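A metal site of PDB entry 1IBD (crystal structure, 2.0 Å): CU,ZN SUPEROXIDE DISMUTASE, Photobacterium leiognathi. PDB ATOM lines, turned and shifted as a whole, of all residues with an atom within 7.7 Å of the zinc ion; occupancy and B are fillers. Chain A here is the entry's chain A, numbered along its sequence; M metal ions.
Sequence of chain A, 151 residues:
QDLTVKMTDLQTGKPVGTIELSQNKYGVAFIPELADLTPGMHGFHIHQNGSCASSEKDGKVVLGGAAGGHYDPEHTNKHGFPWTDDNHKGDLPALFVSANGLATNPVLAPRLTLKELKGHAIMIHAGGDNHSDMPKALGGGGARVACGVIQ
O of His 88 lies within hydrogen-bond range of NH2 of Arg 111.
OD2 of Asp 91 sits at hydrogen-bond distance from ND2 of Asn 87, 2.9 Å away.
The backbone NH of His 88 lies within hydrogen-bond range of the backbone carbonyl oxygen of Lys 78.
OD2 of Asp 133 lies within hydrogen-bond range of N of His 79, at 3.1 Å.
The backbone NH (N) of Gly 80 lies within hydrogen-bond range of the side-chain carboxylate (OD2) of Asp 91, at 3.1 Å.
The backbone NH of His 88 is in hydrogen-bond range of the side-chain hydroxyl of Thr 76 (3.1 Å).
A ring nitrogen (NE2) of His 70 sits close to a ring nitrogen (ND1) of His 45 (3.3 Å).
A ring nitrogen (NE2) of His 79 sits at hydrogen-bond distance from the side-chain carboxylate of Asp 129, 2.7 Å away.
Of the 26 residues printed, 4 come within 4 Å of the zinc ion.
The zinc ion is bound by OD1 of Asp 91 (1.9 Å), ND1 of His 70 (2.1 Å), ND1 of His 79 (2.1 Å) and ND1 of His 88 (2.1 Å).
The zinc ion has four donor atoms within binding distance.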
ATOM      1  N   PHE A  44      -2.266 -19.937  -0.855  1.00  0.00           N
ATOM      2  CA  PHE A  44      -0.824 -19.836  -1.085  1.00  0.00           C
ATOM      3  C   PHE A  44      -0.609 -19.870  -2.606  1.00  0.00           C
ATOM      4  O   PHE A  44      -0.899 -20.866  -3.254  1.00  0.00           O
ATOM      5  CB  PHE A  44      -0.205 -21.064  -0.389  1.00  0.00           C
ATOM      6  CG  PHE A  44       1.295 -21.121  -0.401  1.00  0.00           C
ATOM      7  CD1 PHE A  44       2.075 -19.983  -0.157  1.00  0.00           C
ATOM      8  CD2 PHE A  44       1.934 -22.347  -0.545  1.00  0.00           C
ATOM      9  CE1 PHE A  44       3.458 -20.093  -0.066  1.00  0.00           C
ATOM     10  CE2 PHE A  44       3.311 -22.461  -0.467  1.00  0.00           C
ATOM     11  CZ  PHE A  44       4.078 -21.339  -0.212  1.00  0.00           C
ATOM     12  N   HIS A  45      -0.117 -18.775  -3.186  1.00  0.00           N
ATOM     13  CA  HIS A  45       0.103 -18.742  -4.625  1.00  0.00           C
ATOM     14  C   HIS A  45       1.344 -17.946  -5.033  1.00  0.00           C
ATOM     15  O   HIS A  45       1.843 -17.129  -4.265  1.00  0.00           O
ATOM     16  CB  HIS A  45      -1.104 -18.144  -5.367  1.00  0.00           C
ATOM     17  CG  HIS A  45      -2.410 -18.249  -4.639  1.00  0.00           C
ATOM     18  ND1 HIS A  45      -2.930 -17.210  -3.884  1.00  0.00           N
ATOM     19  CD2 HIS A  45      -3.315 -19.256  -4.559  1.00  0.00           C
ATOM     20  CE1 HIS A  45      -4.078 -17.571  -3.366  1.00  0.00           C
ATOM     21  NE2 HIS A  45      -4.344 -18.815  -3.758  1.00  0.00           N
ATOM     22  N   ILE A  46       1.839 -18.208  -6.237  1.00  0.00           N
ATOM     23  CA  ILE A  46       2.965 -17.447  -6.754  1.00  0.00           C
ATOM     24  C   ILE A  46       2.297 -16.294  -7.503  1.00  0.00           C
ATOM     25  O   ILE A  46       1.291 -16.489  -8.182  1.00  0.00           O
ATOM     26  CB  ILE A  46       3.828 -18.240  -7.784  1.00  0.00           C
ATOM     27  CG1 ILE A  46       4.439 -19.485  -7.143  1.00  0.00           C
ATOM     28  CG2 ILE A  46       4.941 -17.352  -8.338  1.00  0.00           C
ATOM     29  CD1 ILE A  46       5.507 -19.168  -6.088  1.00  0.00           C
ATOM     30  N   HIS A  47       2.841 -15.093  -7.351  1.00  0.00           N
ATOM     31  CA  HIS A  47       2.290 -13.924  -8.020  1.00  0.00           C
ATOM     32  C   HIS A  47       3.122 -13.398  -9.171  1.00  0.00           C
ATOM     33  O   HIS A  47       4.321 -13.667  -9.268  1.00  0.00           O
ATOM     34  CB  HIS A  47       2.025 -12.804  -7.007  1.00  0.00           C
ATOM     35  CG  HIS A  47       0.776 -13.011  -6.219  1.00  0.00           C
ATOM     36  ND1 HIS A  47      -0.273 -12.110  -6.249  1.00  0.00           N
ATOM     37  CD2 HIS A  47       0.364 -14.044  -5.452  1.00  0.00           C
ATOM     38  CE1 HIS A  47      -1.277 -12.592  -5.544  1.00  0.00           C
ATOM     39  NE2 HIS A  47      -0.912 -13.769  -5.048  1.00  0.00           N
ATOM     40  N   GLY A  69      -1.492 -10.017  -9.836  1.00  0.00           N
ATOM     41  CA  GLY A  69      -2.332 -11.195  -9.681  1.00  0.00           C
ATOM     42  C   GLY A  69      -1.580 -12.510  -9.641  1.00  0.00           C
ATOM     43  O   GLY A  69      -0.345 -12.529  -9.601  1.00  0.00           O
ATOM     44  N   HIS A  70      -2.312 -13.622  -9.621  1.00  0.00           N
ATOM     45  CA  HIS A  70      -1.687 -14.932  -9.593  1.00  0.00           C
ATOM     46  C   HIS A  70      -0.851 -15.125 -10.864  1.00  0.00           C
ATOM     47  O   HIS A  70      -1.269 -14.736 -11.952  1.00  0.00           O
ATOM     48  CB  HIS A  70      -2.756 -16.027  -9.499  1.00  0.00           C
ATOM     49  CG  HIS A  70      -3.529 -15.995  -8.226  1.00  0.00           C
ATOM     50  ND1 HIS A  70      -4.438 -16.973  -7.882  1.00  0.00           N
ATOM     51  CD2 HIS A  70      -3.526 -15.111  -7.197  1.00  0.00           C
ATOM     52  CE1 HIS A  70      -4.968 -16.694  -6.700  1.00  0.00           C
ATOM     53  NE2 HIS A  70      -4.433 -15.571  -6.261  1.00  0.00           N
ATOM     54  N   TYR A  71       0.330 -15.711 -10.700  1.00  0.00           N
ATOM     55  CA  TYR A  71       1.228 -15.970 -11.828  1.00  0.00           C
ATOM     56  C   TYR A  71       0.415 -16.761 -12.860  1.00  0.00           C
ATOM     57  O   TYR A  71      -0.061 -17.853 -12.572  1.00  0.00           O
ATOM     58  CB  TYR A  71       2.434 -16.785 -11.311  1.00  0.00           C
ATOM     59  CG  TYR A  71       3.420 -17.249 -12.365  1.00  0.00           C
ATOM     60  CD1 TYR A  71       3.999 -16.347 -13.276  1.00  0.00           C
ATOM     61  CD2 TYR A  71       3.838 -18.585 -12.409  1.00  0.00           C
ATOM     62  CE1 TYR A  71       4.958 -16.776 -14.193  1.00  0.00           C
ATOM     63  CE2 TYR A  71       4.802 -19.012 -13.314  1.00  0.00           C
ATOM     64  CZ  TYR A  71       5.360 -18.101 -14.203  1.00  0.00           C
ATOM     65  OH  TYR A  71       6.309 -18.553 -15.094  1.00  0.00           O
ATOM     66  N   ASP A  72       0.265 -16.196 -14.060  1.00  0.00           N
ATOM     67  CA  ASP A  72      -0.525 -16.827 -15.113  1.00  0.00           C
ATOM     68  C   ASP A  72       0.157 -16.681 -16.477  1.00  0.00           C
ATOM     69  O   ASP A  72      -0.290 -15.925 -17.336  1.00  0.00           O
ATOM     70  CB  ASP A  72      -1.915 -16.179 -15.128  1.00  0.00           C
ATOM     71  CG  ASP A  72      -2.928 -16.926 -16.000  1.00  0.00           C
ATOM     72  OD1 ASP A  72      -2.714 -18.116 -16.300  1.00  0.00           O
ATOM     73  OD2 ASP A  72      -3.953 -16.316 -16.355  1.00  0.00           O
ATOM     74  N   THR A  76      -4.611 -17.932 -18.664  1.00  0.00           N
ATOM     75  CA  THR A  76      -5.814 -18.714 -18.473  1.00  0.00           C
ATOM     76  C   THR A  76      -6.938 -17.857 -17.913  1.00  0.00           C
ATOM     77  O   THR A  76      -8.107 -18.101 -18.178  1.00  0.00           O
ATOM     78  CB  THR A  76      -5.556 -19.873 -17.502  1.00  0.00           C
ATOM     79  OG1 THR A  76      -5.135 -19.346 -16.234  1.00  0.00           O
ATOM     80  CG2 THR A  76      -4.488 -20.806 -18.049  1.00  0.00           C
ATOM     81  N   LYS A  78      -8.051 -17.851 -15.073  1.00  0.00           N
ATOM     82  CA  LYS A  78      -8.880 -18.662 -14.201  1.00  0.00           C
ATOM     83  C   LYS A  78      -8.091 -19.209 -13.020  1.00  0.00           C
ATOM     84  O   LYS A  78      -6.872 -19.369 -13.100  1.00  0.00           O
ATOM     85  CB  LYS A  78      -9.504 -19.822 -14.987  1.00  0.00           C
ATOM     86  CG  LYS A  78     -10.334 -19.373 -16.187  1.00  0.00           C
ATOM     87  CD  LYS A  78     -10.919 -20.543 -16.964  1.00  0.00           C
ATOM     88  CE  LYS A  78     -11.667 -20.061 -18.208  1.00  0.00           C
ATOM     89  NZ  LYS A  78     -12.256 -21.187 -18.979  1.00  0.00           N
ATOM     90  N   HIS A  79      -8.782 -19.490 -11.924  1.00  0.00           N
ATOM     91  CA  HIS A  79      -8.144 -20.019 -10.725  1.00  0.00           C
ATOM     92  C   HIS A  79      -8.580 -21.470 -10.537  1.00  0.00           C
ATOM     93  O   HIS A  79      -9.778 -21.762 -10.523  1.00  0.00           O
ATOM     94  CB  HIS A  79      -8.547 -19.192  -9.502  1.00  0.00           C
ATOM     95  CG  HIS A  79      -7.913 -19.654  -8.224  1.00  0.00           C
ATOM     96  ND1 HIS A  79      -6.582 -19.424  -7.928  1.00  0.00           N
ATOM     97  CD2 HIS A  79      -8.406 -20.355  -7.182  1.00  0.00           C
ATOM     98  CE1 HIS A  79      -6.287 -19.959  -6.765  1.00  0.00           C
ATOM     99  NE2 HIS A  79      -7.384 -20.536  -6.288  1.00  0.00           N
ATOM    100  N   GLY A  80      -7.620 -22.365 -10.377  1.00  0.00           N
ATOM    101  CA  GLY A  80      -7.941 -23.769 -10.211  1.00  0.00           C
ATOM    102  C   GLY A  80      -6.989 -24.568  -9.330  1.00  0.00           C
ATOM    103  O   GLY A  80      -6.418 -24.037  -8.386  1.00  0.00           O
ATOM    104  N   PHE A  81      -6.800 -25.838  -9.660  1.00  0.00           N
ATOM    105  CA  PHE A  81      -5.943 -26.702  -8.879  1.00  0.00           C
ATOM    106  C   PHE A  81      -4.456 -26.690  -9.254  1.00  0.00           C
ATOM    107  O   PHE A  81      -4.051 -26.162 -10.298  1.00  0.00           O
ATOM    108  CB  PHE A  81      -6.482 -28.127  -8.940  1.00  0.00           C
ATOM    109  CG  PHE A  81      -7.865 -28.282  -8.357  1.00  0.00           C
ATOM    110  CD1 PHE A  81      -8.033 -28.645  -7.023  1.00  0.00           C
ATOM    111  CD2 PHE A  81      -8.985 -28.084  -9.152  1.00  0.00           C
ATOM    112  CE1 PHE A  81      -9.316 -28.803  -6.495  1.00  0.00           C
ATOM    113  CE2 PHE A  81     -10.267 -28.233  -8.628  1.00  0.00           C
ATOM    114  CZ  PHE A  81     -10.431 -28.599  -7.302  1.00  0.00           C
ATOM    115  N   ASN A  87      -5.618 -23.088 -15.695  1.00  0.00           N
ATOM    116  CA  ASN A  87      -5.702 -22.079 -14.656  1.00  0.00           C
ATOM    117  C   ASN A  87      -4.318 -21.593 -14.263  1.00  0.00           C
ATOM    118  O   ASN A  87      -3.311 -22.158 -14.689  1.00  0.00           O
ATOM    119  CB  ASN A  87      -6.469 -22.607 -13.428  1.00  0.00           C
ATOM    120  CG  ASN A  87      -5.889 -23.902 -12.888  1.00  0.00           C
ATOM    121  OD1 ASN A  87      -6.273 -24.997 -13.303  1.00  0.00           O
ATOM    122  ND2 ASN A  87      -4.959 -23.777 -11.943  1.00  0.00           N
ATOM    123  N   HIS A  88      -4.267 -20.524 -13.472  1.00  0.00           N
ATOM    124  CA  HIS A  88      -2.998 -19.936 -13.051  1.00  0.00           C
ATOM    125  C   HIS A  88      -1.928 -20.977 -12.723  1.00  0.00           C
ATOM    126  O   HIS A  88      -2.150 -21.863 -11.910  1.00  0.00           O
ATOM    127  CB  HIS A  88      -3.203 -19.056 -11.815  1.00  0.00           C
ATOM    128  CG  HIS A  88      -4.306 -18.061 -11.958  1.00  0.00           C
ATOM    129  ND1 HIS A  88      -5.169 -17.768 -10.917  1.00  0.00           N
ATOM    130  CD2 HIS A  88      -4.681 -17.270 -12.993  1.00  0.00           C
ATOM    131  CE1 HIS A  88      -6.029 -16.849 -11.316  1.00  0.00           C
ATOM    132  NE2 HIS A  88      -5.753 -16.531 -12.564  1.00  0.00           N
ATOM    133  N   LYS A  89      -0.769 -20.854 -13.362  1.00  0.00           N
ATOM    134  CA  LYS A  89       0.316 -21.793 -13.108  1.00  0.00           C
ATOM    135  C   LYS A  89       0.844 -21.545 -11.696  1.00  0.00           C
ATOM    136  O   LYS A  89       1.514 -22.394 -11.118  1.00  0.00           O
ATOM    137  CB  LYS A  89       1.422 -21.578 -14.145  1.00  0.00           C
ATOM    138  CG  LYS A  89       2.261 -22.817 -14.449  1.00  0.00           C
ATOM    139  CD  LYS A  89       3.164 -22.586 -15.652  1.00  0.00           C
ATOM    140  CE  LYS A  89       3.993 -23.822 -15.983  1.00  0.00           C
ATOM    141  NZ  LYS A  89       4.884 -23.591 -17.157  1.00  0.00           N
ATOM    142  N   GLY A  90       0.520 -20.383 -11.137  1.00  0.00           N
ATOM    143  CA  GLY A  90       0.988 -20.069  -9.798  1.00  0.00           C
ATOM    144  C   GLY A  90       0.128 -20.596  -8.658  1.00  0.00           C
ATOM    145  O   GLY A  90       0.439 -20.351  -7.480  1.00  0.00           O
ATOM    146  N   ASP A  91      -0.943 -21.319  -8.990  1.00  0.00           N
ATOM    147  CA  ASP A  91      -1.833 -21.883  -7.978  1.00  0.00           C
ATOM    148  C   ASP A  91      -1.193 -23.046  -7.237  1.00  0.00           C
ATOM    149  O   ASP A  91      -0.992 -24.117  -7.802  1.00  0.00           O
ATOM    150  CB  ASP A  91      -3.144 -22.337  -8.624  1.00  0.00           C
ATOM    151  CG  ASP A  91      -3.900 -21.211  -9.242  1.00  0.00           C
ATOM    152  OD1 ASP A  91      -3.726 -20.073  -8.775  1.00  0.00           O
ATOM    153  OD2 ASP A  91      -4.677 -21.445 -10.196  1.00  0.00           O
ATOM    154  N   LEU A  92      -0.887 -22.855  -5.962  1.00  0.00           N
ATOM    155  CA  LEU A  92      -0.263 -23.909  -5.174  1.00  0.00           C
ATOM    156  C   LEU A  92      -1.240 -24.535  -4.180  1.00  0.00           C
ATOM    157  O   LEU A  92      -2.331 -24.016  -3.960  1.00  0.00           O
ATOM    158  CB  LEU A  92       0.905 -23.306  -4.391  1.00  0.00           C
ATOM    159  CG  LEU A  92       1.807 -22.355  -5.198  1.00  0.00           C
ATOM    160  CD1 LEU A  92       2.621 -21.517  -4.252  1.00  0.00           C
ATOM    161  CD2 LEU A  92       2.700 -23.156  -6.144  1.00  0.00           C
ATOM    162  N   ARG A 111       3.279 -28.436 -11.625  1.00  0.00           N
ATOM    163  CA  ARG A 111       3.317 -27.693 -12.882  1.00  0.00           C
ATOM    164  C   ARG A 111       4.446 -26.665 -13.007  1.00  0.00           C
ATOM    165  O   ARG A 111       4.712 -26.172 -14.102  1.00  0.00           O
ATOM    166  CB  ARG A 111       1.992 -26.976 -13.133  1.00  0.00           C
ATOM    167  CG  ARG A 111       0.885 -27.863 -13.666  1.00  0.00           C
ATOM    168  CD  ARG A 111      -0.308 -27.003 -14.067  1.00  0.00           C
ATOM    169  NE  ARG A 111      -0.946 -26.416 -12.901  1.00  0.00           N
ATOM    170  CZ  ARG A 111      -1.612 -25.258 -12.917  1.00  0.00           C
ATOM    171  NH1 ARG A 111      -1.721 -24.570 -14.050  1.00  0.00           N
ATOM    172  NH2 ARG A 111      -2.175 -24.809 -11.807  1.00  0.00           N
ATOM    173  N   ASP A 129      -8.335 -21.685   0.300  1.00  0.00           N
ATOM    174  CA  ASP A 129      -8.306 -21.821  -1.154  1.00  0.00           C
ATOM    175  C   ASP A 129      -9.043 -23.093  -1.586  1.00  0.00           C
ATOM    176  O   ASP A 129      -8.524 -24.202  -1.411  1.00  0.00           O
ATOM    177  CB  ASP A 129      -6.859 -21.910  -1.627  1.00  0.00           C
ATOM    178  CG  ASP A 129      -6.720 -21.748  -3.146  1.00  0.00           C
ATOM    179  OD1 ASP A 129      -7.740 -21.814  -3.886  1.00  0.00           O
ATOM    180  OD2 ASP A 129      -5.577 -21.569  -3.604  1.00  0.00           O
ATOM    181  N   HIS A 131      -9.706 -23.688  -4.601  1.00  0.00           N
ATOM    182  CA  HIS A 131      -9.289 -23.835  -5.994  1.00  0.00           C
ATOM    183  C   HIS A 131     -10.376 -23.626  -7.020  1.00  0.00           C
ATOM    184  O   HIS A 131     -10.552 -24.440  -7.932  1.00  0.00           O
ATOM    185  CB  HIS A 131      -8.631 -25.194  -6.188  1.00  0.00           C
ATOM    186  CG  HIS A 131      -7.433 -25.397  -5.322  1.00  0.00           C
ATOM    187  ND1 HIS A 131      -7.476 -26.108  -4.134  1.00  0.00           N
ATOM    188  CD2 HIS A 131      -6.180 -24.903  -5.415  1.00  0.00           C
ATOM    189  CE1 HIS A 131      -6.296 -26.037  -3.541  1.00  0.00           C
ATOM    190  NE2 HIS A 131      -5.493 -25.312  -4.292  1.00  0.00           N
ATOM    191  N   SER A 132     -11.084 -22.511  -6.879  1.00  0.00           N
ATOM    192  CA  SER A 132     -12.163 -22.163  -7.789  1.00  0.00           C
ATOM    193  C   SER A 132     -12.445 -20.676  -7.597  1.00  0.00           C
ATOM    194  O   SER A 132     -12.017 -20.090  -6.610  1.00  0.00           O
ATOM    195  CB  SER A 132     -13.417 -22.969  -7.451  1.00  0.00           C
ATOM    196  OG  SER A 132     -14.556 -22.421  -8.066  1.00  0.00           O
ATOM    197  N   ASP A 133     -13.140 -20.076  -8.548  1.00  0.00           N
ATOM    198  CA  ASP A 133     -13.486 -18.666  -8.451  1.00  0.00           C
ATOM    199  C   ASP A 133     -14.886 -18.546  -7.865  1.00  0.00           C
ATOM    200  O   ASP A 133     -15.455 -17.451  -7.793  1.00  0.00           O
ATOM    201  CB  ASP A 133     -13.427 -17.992  -9.825  1.00  0.00           C
ATOM    202  CG  ASP A 133     -12.000 -17.791 -10.314  1.00  0.00           C
ATOM    203  OD1 ASP A 133     -11.230 -17.061  -9.659  1.00  0.00           O
ATOM    204  OD2 ASP A 133     -11.643 -18.361 -11.359  1.00  0.00           O
ATOM    205  N   LEU A 138     -10.627 -16.137  -6.749  1.00  0.00           N
ATOM    206  CA  LEU A 138      -9.301 -16.524  -6.312  1.00  0.00           C
ATOM    207  C   LEU A 138      -9.288 -17.508  -5.144  1.00  0.00           C
ATOM    208  O   LEU A 138      -8.458 -17.411  -4.246  1.00  0.00           O
ATOM    209  CB  LEU A 138      -8.518 -15.259  -5.961  1.00  0.00           C
ATOM    210  CG  LEU A 138      -8.599 -14.139  -7.012  1.00  0.00           C
ATOM    211  CD1 LEU A 138      -7.770 -12.947  -6.581  1.00  0.00           C
ATOM    212  CD2 LEU A 138      -8.116 -14.665  -8.360  1.00  0.00           C
ATOM    213  N   GLY A 139     -10.216 -18.473  -5.169  1.00  0.00           N
ATOM    214  CA  GLY A 139     -10.263 -19.476  -4.113  1.00  0.00           C
ATOM    215  C   GLY A 139     -10.639 -18.970  -2.733  1.00  0.00           C
ATOM    216  O   GLY A 139     -10.540 -19.702  -1.750  1.00  0.00           O
HETATM  217 ZN    ZN M   1      -4.964 -18.648  -8.988  1.00  0.00          ZN
HETATM  218 CU    CU M   2      -2.233 -15.235  -3.907  1.00  0.00          CU
